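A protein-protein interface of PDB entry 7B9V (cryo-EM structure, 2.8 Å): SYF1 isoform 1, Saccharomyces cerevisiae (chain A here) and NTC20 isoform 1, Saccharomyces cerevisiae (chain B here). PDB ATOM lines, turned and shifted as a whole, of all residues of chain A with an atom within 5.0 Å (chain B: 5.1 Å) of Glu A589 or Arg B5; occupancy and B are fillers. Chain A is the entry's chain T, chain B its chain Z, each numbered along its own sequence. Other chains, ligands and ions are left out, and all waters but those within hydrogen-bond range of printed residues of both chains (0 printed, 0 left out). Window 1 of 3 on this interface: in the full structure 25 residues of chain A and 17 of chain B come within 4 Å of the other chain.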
ATOM      1  N   PRO A 585       9.701 -14.735 -15.585  1.00  0.00           N
ATOM      2  CA  PRO A 585       9.845 -15.413 -14.279  1.00  0.00           C
ATOM      3  C   PRO A 585      11.023 -16.366 -14.192  1.00  0.00           C
ATOM      4  O   PRO A 585      11.748 -16.373 -13.181  1.00  0.00           O
ATOM      5  CB  PRO A 585       8.512 -16.148 -14.127  1.00  0.00           C
ATOM      6  CG  PRO A 585       7.600 -15.306 -14.866  1.00  0.00           C
ATOM      7  CD  PRO A 585       8.301 -14.804 -16.035  1.00  0.00           C
ATOM      8  N   ALA A 586      11.216 -17.179 -15.236  1.00  0.00           N
ATOM      9  CA  ALA A 586      12.316 -18.129 -15.233  1.00  0.00           C
ATOM     10  C   ALA A 586      13.654 -17.415 -15.301  1.00  0.00           C
ATOM     11  O   ALA A 586      14.594 -17.826 -14.629  1.00  0.00           O
ATOM     12  CB  ALA A 586      12.172 -19.106 -16.397  1.00  0.00           C
ATOM     13  N   MET A 587      13.731 -16.291 -16.034  1.00  0.00           N
ATOM     14  CA  MET A 587      14.962 -15.501 -16.081  1.00  0.00           C
ATOM     15  C   MET A 587      15.261 -14.823 -14.746  1.00  0.00           C
ATOM     16  O   MET A 587      16.434 -14.645 -14.386  1.00  0.00           O
ATOM     17  CB  MET A 587      14.861 -14.450 -17.189  1.00  0.00           C
ATOM     18  CG  MET A 587      16.163 -13.754 -17.541  1.00  0.00           C
ATOM     19  SD  MET A 587      15.977 -12.635 -18.936  1.00  0.00           S
ATOM     20  CE  MET A 587      15.702 -13.812 -20.251  1.00  0.00           C
ATOM     21  N   ALA A 588      14.218 -14.505 -13.975  1.00  0.00           N
ATOM     22  CA  ALA A 588      14.418 -13.933 -12.649  1.00  0.00           C
ATOM     23  C   ALA A 588      14.964 -14.979 -11.694  1.00  0.00           C
ATOM     24  O   ALA A 588      15.872 -14.696 -10.895  1.00  0.00           O
ATOM     25  CB  ALA A 588      13.109 -13.355 -12.120  1.00  0.00           C
ATOM     26  N   GLU A 589      14.385 -16.187 -11.744  1.00  0.00           N
ATOM     27  CA  GLU A 589      14.924 -17.293 -10.962  1.00  0.00           C
ATOM     28  C   GLU A 589      16.347 -17.659 -11.417  1.00  0.00           C
ATOM     29  O   GLU A 589      17.169 -18.069 -10.586  1.00  0.00           O
ATOM     30  CB  GLU A 589      13.976 -18.504 -11.038  1.00  0.00           C
ATOM     31  CG  GLU A 589      14.476 -19.822 -10.405  1.00  0.00           C
ATOM     32  CD  GLU A 589      14.908 -19.727  -8.915  1.00  0.00           C
ATOM     33  OE1 GLU A 589      14.477 -18.825  -8.158  1.00  0.00           O
ATOM     34  OE2 GLU A 589      15.761 -20.540  -8.503  1.00  0.00           O
ATOM     35  N   ASN A 590      16.671 -17.463 -12.714  1.00  0.00           N
ATOM     36  CA  ASN A 590      18.045 -17.657 -13.187  1.00  0.00           C
ATOM     37  C   ASN A 590      18.988 -16.652 -12.547  1.00  0.00           C
ATOM     38  O   ASN A 590      20.124 -17.003 -12.205  1.00  0.00           O
ATOM     39  CB  ASN A 590      18.138 -17.521 -14.712  1.00  0.00           C
ATOM     40  CG  ASN A 590      17.415 -18.615 -15.458  1.00  0.00           C
ATOM     41  OD1 ASN A 590      17.055 -19.622 -14.876  1.00  0.00           O
ATOM     42  ND2 ASN A 590      17.158 -18.401 -16.747  1.00  0.00           N
ATOM     43  N   PHE A 591      18.553 -15.384 -12.441  1.00  0.00           N
ATOM     44  CA  PHE A 591      19.367 -14.360 -11.779  1.00  0.00           C
ATOM     45  C   PHE A 591      19.601 -14.714 -10.316  1.00  0.00           C
ATOM     46  O   PHE A 591      20.715 -14.542  -9.795  1.00  0.00           O
ATOM     47  CB  PHE A 591      18.658 -13.002 -11.912  1.00  0.00           C
ATOM     48  CG  PHE A 591      19.500 -11.781 -11.543  1.00  0.00           C
ATOM     49  CD1 PHE A 591      20.886 -11.832 -11.426  1.00  0.00           C
ATOM     50  CD2 PHE A 591      18.874 -10.552 -11.356  1.00  0.00           C
ATOM     51  CE1 PHE A 591      21.617 -10.716 -11.079  1.00  0.00           C
ATOM     52  CE2 PHE A 591      19.605  -9.419 -11.023  1.00  0.00           C
ATOM     53  CZ  PHE A 591      20.978  -9.507 -10.878  1.00  0.00           C
ATOM     54  N   ALA A 592      18.549 -15.206  -9.648  1.00  0.00           N
ATOM     55  CA  ALA A 592      18.668 -15.599  -8.250  1.00  0.00           C
ATOM     56  C   ALA A 592      19.638 -16.754  -8.071  1.00  0.00           C
ATOM     57  O   ALA A 592      20.461 -16.745  -7.148  1.00  0.00           O
ATOM     58  CB  ALA A 592      17.302 -15.968  -7.713  1.00  0.00           C
ATOM     59  N   LEU A 593      19.538 -17.767  -8.945  1.00  0.00           N
ATOM     60  CA  LEU A 593      20.418 -18.922  -8.834  1.00  0.00           C
ATOM     61  C   LEU A 593      21.850 -18.559  -9.175  1.00  0.00           C
ATOM     62  O   LEU A 593      22.780 -19.140  -8.609  1.00  0.00           O
ATOM     63  CB  LEU A 593      19.940 -20.050  -9.741  1.00  0.00           C
ATOM     64  CG  LEU A 593      20.429 -21.447  -9.365  1.00  0.00           C
ATOM     65  CD1 LEU A 593      19.568 -22.023  -8.267  1.00  0.00           C
ATOM     66  CD2 LEU A 593      20.439 -22.362 -10.578  1.00  0.00           C
ATOM     67  N   PHE A 594      22.031 -17.613 -10.109  1.00  0.00           N
ATOM     68  CA  PHE A 594      23.357 -17.107 -10.429  1.00  0.00           C
ATOM     69  C   PHE A 594      23.997 -16.454  -9.220  1.00  0.00           C
ATOM     70  O   PHE A 594      25.173 -16.695  -8.918  1.00  0.00           O
ATOM     71  CB  PHE A 594      23.265 -16.116 -11.582  1.00  0.00           C
ATOM     72  CG  PHE A 594      24.559 -15.442 -11.892  1.00  0.00           C
ATOM     73  CD1 PHE A 594      25.600 -16.152 -12.462  1.00  0.00           C
ATOM     74  CD2 PHE A 594      24.749 -14.104 -11.584  1.00  0.00           C
ATOM     75  CE1 PHE A 594      26.802 -15.536 -12.739  1.00  0.00           C
ATOM     76  CE2 PHE A 594      25.944 -13.482 -11.854  1.00  0.00           C
ATOM     77  CZ  PHE A 594      26.974 -14.198 -12.433  1.00  0.00           C
ATOM     78  N   GLN A 596      23.158 -16.819  -6.054  1.00  0.00           N
ATOM     79  CA  GLN A 596      23.354 -17.791  -4.984  1.00  0.00           C
ATOM     80  C   GLN A 596      24.578 -18.665  -5.226  1.00  0.00           C
ATOM     81  O   GLN A 596      25.273 -19.031  -4.271  1.00  0.00           O
ATOM     82  CB  GLN A 596      22.111 -18.658  -4.826  1.00  0.00           C
ATOM     83  CG  GLN A 596      21.017 -18.025  -4.008  1.00  0.00           C
ATOM     84  CD  GLN A 596      19.642 -18.341  -4.542  1.00  0.00           C
ATOM     85  OE1 GLN A 596      18.845 -17.446  -4.804  1.00  0.00           O
ATOM     86  NE2 GLN A 596      19.365 -19.623  -4.728  1.00  0.00           N
ATOM     87  N   TYR A 608      14.548 -11.389  -5.637  1.00  0.00           N
ATOM     88  CA  TYR A 608      13.191 -11.903  -5.456  1.00  0.00           C
ATOM     89  C   TYR A 608      12.249 -10.767  -5.093  1.00  0.00           C
ATOM     90  O   TYR A 608      11.129 -10.712  -5.600  1.00  0.00           O
ATOM     91  CB  TYR A 608      13.144 -13.006  -4.399  1.00  0.00           C
ATOM     92  CG  TYR A 608      13.721 -14.334  -4.816  1.00  0.00           C
ATOM     93  CD1 TYR A 608      13.346 -14.938  -6.013  1.00  0.00           C
ATOM     94  CD2 TYR A 608      14.612 -14.999  -3.995  1.00  0.00           C
ATOM     95  CE1 TYR A 608      13.872 -16.163  -6.383  1.00  0.00           C
ATOM     96  CE2 TYR A 608      15.134 -16.217  -4.350  1.00  0.00           C
ATOM     97  CZ  TYR A 608      14.757 -16.801  -5.536  1.00  0.00           C
ATOM     98  OH  TYR A 608      15.292 -18.021  -5.880  1.00  0.00           O
ATOM     99  N   LEU A 623       7.534 -18.274  -7.499  1.00  0.00           N
ATOM    100  CA  LEU A 623       8.721 -17.548  -7.072  1.00  0.00           C
ATOM    101  C   LEU A 623       8.870 -17.525  -5.565  1.00  0.00           C
ATOM    102  O   LEU A 623       9.997 -17.535  -5.057  1.00  0.00           O
ATOM    103  CB  LEU A 623       8.689 -16.110  -7.610  1.00  0.00           C
ATOM    104  CG  LEU A 623       9.252 -15.861  -9.014  1.00  0.00           C
ATOM    105  CD1 LEU A 623       8.882 -14.466  -9.470  1.00  0.00           C
ATOM    106  CD2 LEU A 623      10.762 -16.059  -9.055  1.00  0.00           C
ATOM    107  N   GLU A 626      10.510 -20.534  -4.207  1.00  0.00           N
ATOM    108  CA  GLU A 626      11.959 -20.419  -4.319  1.00  0.00           C
ATOM    109  C   GLU A 626      12.543 -19.586  -3.202  1.00  0.00           C
ATOM    110  O   GLU A 626      13.519 -19.990  -2.556  1.00  0.00           O
ATOM    111  CB  GLU A 626      12.390 -19.818  -5.661  1.00  0.00           C
ATOM    112  CG  GLU A 626      11.805 -20.423  -6.894  1.00  0.00           C
ATOM    113  CD  GLU A 626      12.110 -21.902  -7.096  1.00  0.00           C
ATOM    114  OE1 GLU A 626      13.052 -22.467  -6.501  1.00  0.00           O
ATOM    115  OE2 GLU A 626      11.392 -22.502  -7.914  1.00  0.00           O
ATOM    116  N   PRO B   2      10.345 -27.533  -6.090  1.00  0.00           N
ATOM    117  CA  PRO B   2       9.956 -26.255  -6.694  1.00  0.00           C
ATOM    118  C   PRO B   2       9.920 -26.326  -8.218  1.00  0.00           C
ATOM    119  O   PRO B   2      10.529 -27.213  -8.804  1.00  0.00           O
ATOM    120  CB  PRO B   2      11.055 -25.298  -6.224  1.00  0.00           C
ATOM    121  CG  PRO B   2      11.579 -25.915  -4.981  1.00  0.00           C
ATOM    122  CD  PRO B   2      11.534 -27.394  -5.235  1.00  0.00           C
ATOM    123  N   SER B   3       9.191 -25.404  -8.846  1.00  0.00           N
ATOM    124  CA  SER B   3       8.946 -25.461 -10.284  1.00  0.00           C
ATOM    125  C   SER B   3      10.032 -24.773 -11.102  1.00  0.00           C
ATOM    126  O   SER B   3      10.534 -25.346 -12.067  1.00  0.00           O
ATOM    127  CB  SER B   3       7.598 -24.847 -10.638  1.00  0.00           C
ATOM    128  OG  SER B   3       6.548 -25.481  -9.930  1.00  0.00           O
ATOM    129  N   LEU B   4      10.327 -23.509 -10.794  1.00  0.00           N
ATOM    130  CA  LEU B   4      11.258 -22.735 -11.609  1.00  0.00           C
ATOM    131  C   LEU B   4      12.714 -23.150 -11.423  1.00  0.00           C
ATOM    132  O   LEU B   4      13.541 -22.892 -12.317  1.00  0.00           O
ATOM    133  CB  LEU B   4      11.112 -21.251 -11.271  1.00  0.00           C
ATOM    134  CG  LEU B   4       9.829 -20.537 -11.671  1.00  0.00           C
ATOM    135  CD1 LEU B   4       9.770 -19.174 -11.039  1.00  0.00           C
ATOM    136  CD2 LEU B   4       9.837 -20.393 -13.160  1.00  0.00           C
ATOM    137  N   ARG B   5      13.050 -23.731 -10.261  1.00  0.00           N
ATOM    138  CA  ARG B   5      14.445 -24.000  -9.901  1.00  0.00           C
ATOM    139  C   ARG B   5      15.098 -24.993 -10.855  1.00  0.00           C
ATOM    140  O   ARG B   5      16.232 -24.788 -11.290  1.00  0.00           O
ATOM    141  CB  ARG B   5      14.555 -24.514  -8.474  1.00  0.00           C
ATOM    142  CG  ARG B   5      15.962 -24.359  -7.925  1.00  0.00           C
ATOM    143  CD  ARG B   5      16.116 -24.829  -6.488  1.00  0.00           C
ATOM    144  NE  ARG B   5      17.301 -24.237  -5.872  1.00  0.00           N
ATOM    145  CZ  ARG B   5      18.551 -24.652  -6.033  1.00  0.00           C
ATOM    146  NH1 ARG B   5      18.846 -25.692  -6.795  1.00  0.00           N
ATOM    147  NH2 ARG B   5      19.533 -24.000  -5.417  1.00  0.00           N
ATOM    148  N   ASP B   6      14.439 -26.126 -11.112  1.00  0.00           N
ATOM    149  CA  ASP B   6      15.077 -27.133 -11.951  1.00  0.00           C
ATOM    150  C   ASP B   6      15.089 -26.737 -13.424  1.00  0.00           C
ATOM    151  O   ASP B   6      15.925 -27.249 -14.169  1.00  0.00           O
ATOM    152  CB  ASP B   6      14.431 -28.510 -11.741  1.00  0.00           C
ATOM    153  CG  ASP B   6      12.923 -28.521 -11.970  1.00  0.00           C
ATOM    154  OD1 ASP B   6      12.336 -27.518 -12.408  1.00  0.00           O
ATOM    155  OD2 ASP B   6      12.310 -29.574 -11.697  1.00  0.00           O
ATOM    156  N   LEU B   7      14.166 -25.860 -13.852  1.00  0.00           N
ATOM    157  CA  LEU B   7      14.310 -25.197 -15.148  1.00  0.00           C
ATOM    158  C   LEU B   7      15.602 -24.404 -15.190  1.00  0.00           C
ATOM    159  O   LEU B   7      16.339 -24.450 -16.192  1.00  0.00           O
ATOM    160  CB  LEU B   7      13.132 -24.274 -15.432  1.00  0.00           C
ATOM    161  CG  LEU B   7      11.714 -24.812 -15.334  1.00  0.00           C
ATOM    162  CD1 LEU B   7      10.788 -23.705 -15.743  1.00  0.00           C
ATOM    163  CD2 LEU B   7      11.512 -26.030 -16.208  1.00  0.00           C
ATOM    164  N   SER B   8      15.891 -23.670 -14.100  1.00  0.00           N
ATOM    165  CA  SER B   8      17.138 -22.913 -14.042  1.00  0.00           C
ATOM    166  C   SER B   8      18.346 -23.840 -14.030  1.00  0.00           C
ATOM    167  O   SER B   8      19.373 -23.527 -14.642  1.00  0.00           O
ATOM    168  CB  SER B   8      17.171 -22.050 -12.782  1.00  0.00           C
ATOM    169  OG  SER B   8      18.218 -21.096 -12.876  1.00  0.00           O
ATOM    170  N   LEU B   9      18.242 -24.966 -13.313  1.00  0.00           N
ATOM    171  CA  LEU B   9      19.348 -25.918 -13.226  1.00  0.00           C
ATOM    172  C   LEU B   9      19.640 -26.554 -14.580  1.00  0.00           C
ATOM    173  O   LEU B   9      20.808 -26.774 -14.934  1.00  0.00           O
ATOM    174  CB  LEU B   9      19.048 -26.992 -12.183  1.00  0.00           C
ATOM    175  CG  LEU B   9      19.069 -26.640 -10.697  1.00  0.00           C
ATOM    176  CD1 LEU B   9      18.413 -27.748  -9.885  1.00  0.00           C
ATOM    177  CD2 LEU B   9      20.497 -26.400 -10.230  1.00  0.00           C
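Among the printed residues, merely in contact across the chains: Glu A626 with Pro B2 (3.3 Å), Leu A593 with Ser B8 (3.4 Å), Leu A593 with Arg B5 (3.5 Å), Glu A589 with Leu B4 (3.7 Å), Glu A626 with Ser B3 (3.8 Å), Leu A623 with Leu B4 (3.8 Å), Glu A589 with Arg B5 (3.9 Å), Glu A589 with Ser B8 (3.9 Å) and Ala A586 with Leu B4 (3.9 Å).
OD1 of Asn A590 sits at hydrogen-bond distance from OG of Ser B8 (2.7 Å).
OE2 of Glu A626 lies within hydrogen-bond range of N of Leu B4.
N of Arg B5 lies within hydrogen-bond range of OE2 of Glu A626.
Glu A589 touches three residues of chain B.
Printed residues of chain A within 4 Å of Ser B8: Glu A589 (3.9 Å), Asn A590 (2.7 Å) and Leu A593 (3.4 Å).
Of the printed residues of chain B, Leu A623 touches Leu B4.
Of the printed residues of chain B, Asn A590 touches Ser B8.
Of the printed residues of chain A, Ser B3 touches Glu A626.
Gln A596 touches none of the printed residues of chain B.
Tyr A608 touches none of the printed residues of chain B.
The nearest residue of chain A that does not touch Arg B5 is Gln A596 (4.4 Å).
The nearest printed residue of chain B that does not touch Glu A626 is Asp B6 (5.7 Å).
Of the 14 printed residues of chain A, 6 touch a printed residue of chain B.
Printed residues of chain A that touch a printed residue of chain B: Ala A586, Glu A589, Asn A590, Leu A593, Leu A623 and Glu A626.
Hydrophobic or aromatic side chains of chain A within 4 Å of the printed part of chain B: Leu A593 and Leu A623.
The backbone carbonyl oxygen (O) of Ala A586 sits close to the side-chain amide oxygen (OD1) of Asn A590 (3.1 Å).
OE1 of Glu A589 sits at hydrogen-bond distance from OH of Tyr A608 (2.5 Å).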
